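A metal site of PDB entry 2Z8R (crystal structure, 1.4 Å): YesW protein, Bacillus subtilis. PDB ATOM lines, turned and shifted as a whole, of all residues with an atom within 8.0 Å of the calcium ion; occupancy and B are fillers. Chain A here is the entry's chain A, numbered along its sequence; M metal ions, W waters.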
ATOM      1  N   ASN A   9      18.463 -23.639  20.858  1.00  0.00           N
ATOM      2  CA  ASN A   9      17.308 -23.469  21.728  1.00  0.00           C
ATOM      3  C   ASN A   9      16.242 -24.508  21.339  1.00  0.00           C
ATOM      4  O   ASN A   9      16.535 -25.427  20.564  1.00  0.00           O
ATOM      5  CB  ASN A   9      16.801 -22.005  21.728  1.00  0.00           C
ATOM      6  CG  ASN A   9      16.114 -21.596  20.439  1.00  0.00           C
ATOM      7  OD1 ASN A   9      15.868 -22.408  19.544  1.00  0.00           O
ATOM      8  ND2 ASN A   9      15.763 -20.301  20.342  1.00  0.00           N
ATOM      9  N   GLY A 120      23.888 -19.903  10.374  1.00  0.00           N
ATOM     10  CA  GLY A 120      24.761 -20.040  11.528  1.00  0.00           C
ATOM     11  C   GLY A 120      24.135 -19.231  12.647  1.00  0.00           C
ATOM     12  O   GLY A 120      23.353 -18.332  12.395  1.00  0.00           O
ATOM     13  N   ASP A 121      24.505 -19.556  13.876  1.00  0.00           N
ATOM     14  CA  ASP A 121      24.038 -18.789  15.015  1.00  0.00           C
ATOM     15  C   ASP A 121      25.163 -17.815  15.369  1.00  0.00           C
ATOM     16  O   ASP A 121      26.134 -18.186  16.031  1.00  0.00           O
ATOM     17  CB  ASP A 121      23.728 -19.729  16.187  1.00  0.00           C
ATOM     18  CG  ASP A 121      23.247 -18.997  17.424  1.00  0.00           C
ATOM     19  OD1 ASP A 121      22.891 -17.809  17.312  1.00  0.00           O
ATOM     20  OD2 ASP A 121      23.229 -19.620  18.497  1.00  0.00           O
ATOM     21  N   VAL A 122      25.041 -16.583  14.877  1.00  0.00           N
ATOM     22  CA  VAL A 122      26.144 -15.627  14.985  1.00  0.00           C
ATOM     23  C   VAL A 122      26.239 -14.958  16.358  1.00  0.00           C
ATOM     24  O   VAL A 122      27.292 -14.408  16.705  1.00  0.00           O
ATOM     25  CB  VAL A 122      26.090 -14.545  13.870  1.00  0.00           C
ATOM     26  CG1 VAL A 122      26.023 -15.195  12.491  1.00  0.00           C
ATOM     27  CG2 VAL A 122      24.932 -13.558  14.095  1.00  0.00           C
ATOM     28  N   ASP A 123      25.164 -15.015  17.128  1.00  0.00           N
ATOM     29  CA  ASP A 123      25.147 -14.372  18.445  1.00  0.00           C
ATOM     30  C   ASP A 123      25.009 -15.350  19.619  1.00  0.00           C
ATOM     31  O   ASP A 123      25.049 -14.931  20.772  1.00  0.00           O
ATOM     32  CB  ASP A 123      24.108 -13.230  18.521  1.00  0.00           C
ATOM     33  CG  ASP A 123      22.696 -13.677  18.210  1.00  0.00           C
ATOM     34  OD1 ASP A 123      22.484 -14.834  17.781  1.00  0.00           O
ATOM     35  OD2 ASP A 123      21.778 -12.843  18.371  1.00  0.00           O
ATOM     36  N   GLY A 124      24.854 -16.645  19.323  1.00  0.00           N
ATOM     37  CA  GLY A 124      24.945 -17.674  20.355  1.00  0.00           C
ATOM     38  C   GLY A 124      23.697 -17.914  21.195  1.00  0.00           C
ATOM     39  O   GLY A 124      23.782 -18.524  22.263  1.00  0.00           O
ATOM     40  N   ASP A 125      22.541 -17.478  20.702  1.00  0.00           N
ATOM     41  CA  ASP A 125      21.289 -17.667  21.453  1.00  0.00           C
ATOM     42  C   ASP A 125      20.535 -18.950  21.087  1.00  0.00           C
ATOM     43  O   ASP A 125      19.461 -19.229  21.626  1.00  0.00           O
ATOM     44  CB  ASP A 125      20.364 -16.446  21.306  1.00  0.00           C
ATOM     45  CG  ASP A 125      19.802 -16.302  19.902  1.00  0.00           C
ATOM     46  OD1 ASP A 125      20.315 -16.937  18.946  1.00  0.00           O
ATOM     47  OD2 ASP A 125      18.826 -15.530  19.740  1.00  0.00           O
ATOM     48  N   GLY A 126      21.093 -19.739  20.171  1.00  0.00           N
ATOM     49  CA  GLY A 126      20.463 -21.013  19.802  1.00  0.00           C
ATOM     50  C   GLY A 126      19.413 -20.944  18.702  1.00  0.00           C
ATOM     51  O   GLY A 126      18.771 -21.948  18.392  1.00  0.00           O
ATOM     52  N   GLN A 127      19.246 -19.759  18.121  1.00  0.00           N
ATOM     53  CA  GLN A 127      18.395 -19.551  16.943  1.00  0.00           C
ATOM     54  C   GLN A 127      19.279 -19.180  15.756  1.00  0.00           C
ATOM     55  O   GLN A 127      20.141 -18.304  15.878  1.00  0.00           O
ATOM     56  CB  GLN A 127      17.381 -18.442  17.214  1.00  0.00           C
ATOM     57  CG  GLN A 127      16.470 -18.180  16.030  1.00  0.00           C
ATOM     58  CD  GLN A 127      15.474 -17.086  16.282  1.00  0.00           C
ATOM     59  OE1 GLN A 127      14.443 -17.309  16.910  1.00  0.00           O
ATOM     60  NE2 GLN A 127      15.761 -15.888  15.763  1.00  0.00           N
ATOM     61  N   TYR A 128      19.079 -19.820  14.601  1.00  0.00           N
ATOM     62  CA  TYR A 128      19.904 -19.532  13.422  1.00  0.00           C
ATOM     63  C   TYR A 128      19.598 -18.171  12.810  1.00  0.00           C
ATOM     64  O   TYR A 128      18.423 -17.760  12.717  1.00  0.00           O
ATOM     65  CB  TYR A 128      19.697 -20.606  12.351  1.00  0.00           C
ATOM     66  CG  TYR A 128      20.287 -21.936  12.711  1.00  0.00           C
ATOM     67  CD1 TYR A 128      21.678 -22.086  12.844  1.00  0.00           C
ATOM     68  CD2 TYR A 128      19.477 -23.056  12.919  1.00  0.00           C
ATOM     69  CE1 TYR A 128      22.231 -23.303  13.193  1.00  0.00           C
ATOM     70  CE2 TYR A 128      20.034 -24.282  13.268  1.00  0.00           C
ATOM     71  CZ  TYR A 128      21.413 -24.394  13.401  1.00  0.00           C
ATOM     72  OH  TYR A 128      21.947 -25.606  13.728  1.00  0.00           O
ATOM     73  N   GLU A 129      20.667 -17.504  12.366  1.00  0.00           N
ATOM     74  CA  GLU A 129      20.573 -16.402  11.408  1.00  0.00           C
ATOM     75  C   GLU A 129      20.715 -16.962   9.990  1.00  0.00           C
ATOM     76  O   GLU A 129      21.303 -18.043   9.805  1.00  0.00           O
ATOM     77  CB  GLU A 129      21.703 -15.395  11.653  1.00  0.00           C
ATOM     78  CG  GLU A 129      21.457 -14.449  12.839  1.00  0.00           C
ATOM     79  CD  GLU A 129      21.351 -15.184  14.179  1.00  0.00           C
ATOM     80  OE1 GLU A 129      22.311 -15.865  14.605  1.00  0.00           O
ATOM     81  OE2 GLU A 129      20.295 -15.025  14.839  1.00  0.00           O
ATOM     82  N   LEU A 130      20.180 -16.227   9.018  1.00  0.00           N
ATOM     83  CA  LEU A 130      20.347 -16.547   7.614  1.00  0.00           C
ATOM     84  C   LEU A 130      21.462 -15.696   7.022  1.00  0.00           C
ATOM     85  O   LEU A 130      21.467 -14.472   7.193  1.00  0.00           O
ATOM     86  CB  LEU A 130      19.048 -16.296   6.851  1.00  0.00           C
ATOM     87  CG  LEU A 130      17.984 -17.363   7.078  1.00  0.00           C
ATOM     88  CD1 LEU A 130      16.578 -16.818   6.807  1.00  0.00           C
ATOM     89  CD2 LEU A 130      18.256 -18.604   6.236  1.00  0.00           C
ATOM     90  N   TYR A 156      20.898 -11.865   8.211  1.00  0.00           N
ATOM     91  CA  TYR A 156      19.586 -11.485   8.745  1.00  0.00           C
ATOM     92  C   TYR A 156      19.213 -12.340   9.932  1.00  0.00           C
ATOM     93  O   TYR A 156      19.377 -13.561   9.905  1.00  0.00           O
ATOM     94  CB  TYR A 156      18.496 -11.671   7.690  1.00  0.00           C
ATOM     95  CG  TYR A 156      18.601 -10.704   6.552  1.00  0.00           C
ATOM     96  CD1 TYR A 156      17.988  -9.453   6.599  1.00  0.00           C
ATOM     97  CD2 TYR A 156      19.325 -11.050   5.394  1.00  0.00           C
ATOM     98  CE1 TYR A 156      18.104  -8.556   5.540  1.00  0.00           C
ATOM     99  CE2 TYR A 156      19.444 -10.162   4.335  1.00  0.00           C
ATOM    100  CZ  TYR A 156      18.832  -8.921   4.403  1.00  0.00           C
ATOM    101  OH  TYR A 156      18.965  -8.050   3.355  1.00  0.00           O
ATOM    102  N   LYS A 157      18.676 -11.702  10.966  1.00  0.00           N
ATOM    103  CA  LYS A 157      17.957 -12.441  12.009  1.00  0.00           C
ATOM    104  C   LYS A 157      16.593 -12.831  11.465  1.00  0.00           C
ATOM    105  O   LYS A 157      16.098 -12.220  10.503  1.00  0.00           O
ATOM    106  CB  LYS A 157      17.809 -11.599  13.266  1.00  0.00           C
ATOM    107  CG  LYS A 157      19.151 -11.299  13.945  1.00  0.00           C
ATOM    108  CD  LYS A 157      18.953 -10.642  15.308  1.00  0.00           C
ATOM    109  CE  LYS A 157      18.641 -11.667  16.396  1.00  0.00           C
ATOM    110  NZ  LYS A 157      19.853 -12.476  16.771  1.00  0.00           N
ATOM    111  N   LEU A 158      15.973 -13.834  12.067  1.00  0.00           N
ATOM    112  CA  LEU A 158      14.691 -14.292  11.551  1.00  0.00           C
ATOM    113  C   LEU A 158      13.582 -13.236  11.645  1.00  0.00           C
ATOM    114  O   LEU A 158      12.624 -13.272  10.877  1.00  0.00           O
ATOM    115  CB  LEU A 158      14.262 -15.621  12.176  1.00  0.00           C
ATOM    116  CG  LEU A 158      15.221 -16.811  12.026  1.00  0.00           C
ATOM    117  CD1 LEU A 158      14.558 -18.092  12.541  1.00  0.00           C
ATOM    118  CD2 LEU A 158      15.720 -16.990  10.582  1.00  0.00           C
ATOM    119  N   LEU A 163      21.801  -7.555   9.912  1.00  0.00           N
ATOM    120  CA  LEU A 163      22.971  -7.354  10.746  1.00  0.00           C
ATOM    121  C   LEU A 163      24.131  -6.679  10.032  1.00  0.00           C
ATOM    122  O   LEU A 163      24.849  -5.880  10.647  1.00  0.00           O
ATOM    123  CB  LEU A 163      23.442  -8.670  11.373  1.00  0.00           C
ATOM    124  CG  LEU A 163      22.406  -9.399  12.233  1.00  0.00           C
ATOM    125  CD1 LEU A 163      22.951 -10.712  12.708  1.00  0.00           C
ATOM    126  CD2 LEU A 163      21.997  -8.548  13.434  1.00  0.00           C
ATOM    127  N   GLY A 190      30.897 -20.708  20.436  1.00  0.00           N
ATOM    128  CA  GLY A 190      29.437 -20.696  20.430  1.00  0.00           C
ATOM    129  C   GLY A 190      28.793 -19.766  19.400  1.00  0.00           C
ATOM    130  O   GLY A 190      27.572 -19.717  19.276  1.00  0.00           O
HETATM  131 CA    CA M   1      21.059 -16.332  16.759  1.00  0.00          CA
HETATM  132  O   HOH W   1      18.891 -15.183  17.248  1.00  0.00           O
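Water W1 lies within hydrogen-bond range of the side-chain carboxylate of Asp 125 (2.5 Å) and the side-chain amino group of Lys 157 (2.9 Å).
OD2 of Asp 123 is in salt-bridge range of NZ of Lys 157. The backbone carbonyl oxygen (O) of Gly 120 sits at hydrogen-bond distance from the backbone NH (N) of Glu 129 (2.8 Å). N of Val 122 sits close to OE1 of Glu 129 (2.8 Å). The side-chain carboxylate (OD2) of Asp 121 sits close to the backbone NH (N) of Gly 124. OE2 of Glu 129 sits close to NZ of Lys 157 (3.2 Å). N of Gly 126 sits at hydrogen-bond distance from OD2 of Asp 121 (2.7 Å).
Along chain A the residues within 4 Å of the calcium ion span positions 121 to 129.
The calcium ion is bound by OD1 of Asp 123 (2.3 Å), O of Gln 127 (2.3 Å), OD1 of Asp 125 (2.4 Å), OD1 of Asp 121 (2.4 Å), OE2 of Glu 129 (2.4 Å), water W1 (2.5 Å) and OE1 of Glu 129 (2.5 Å). The calcium ion has seven donor atoms within binding distance.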
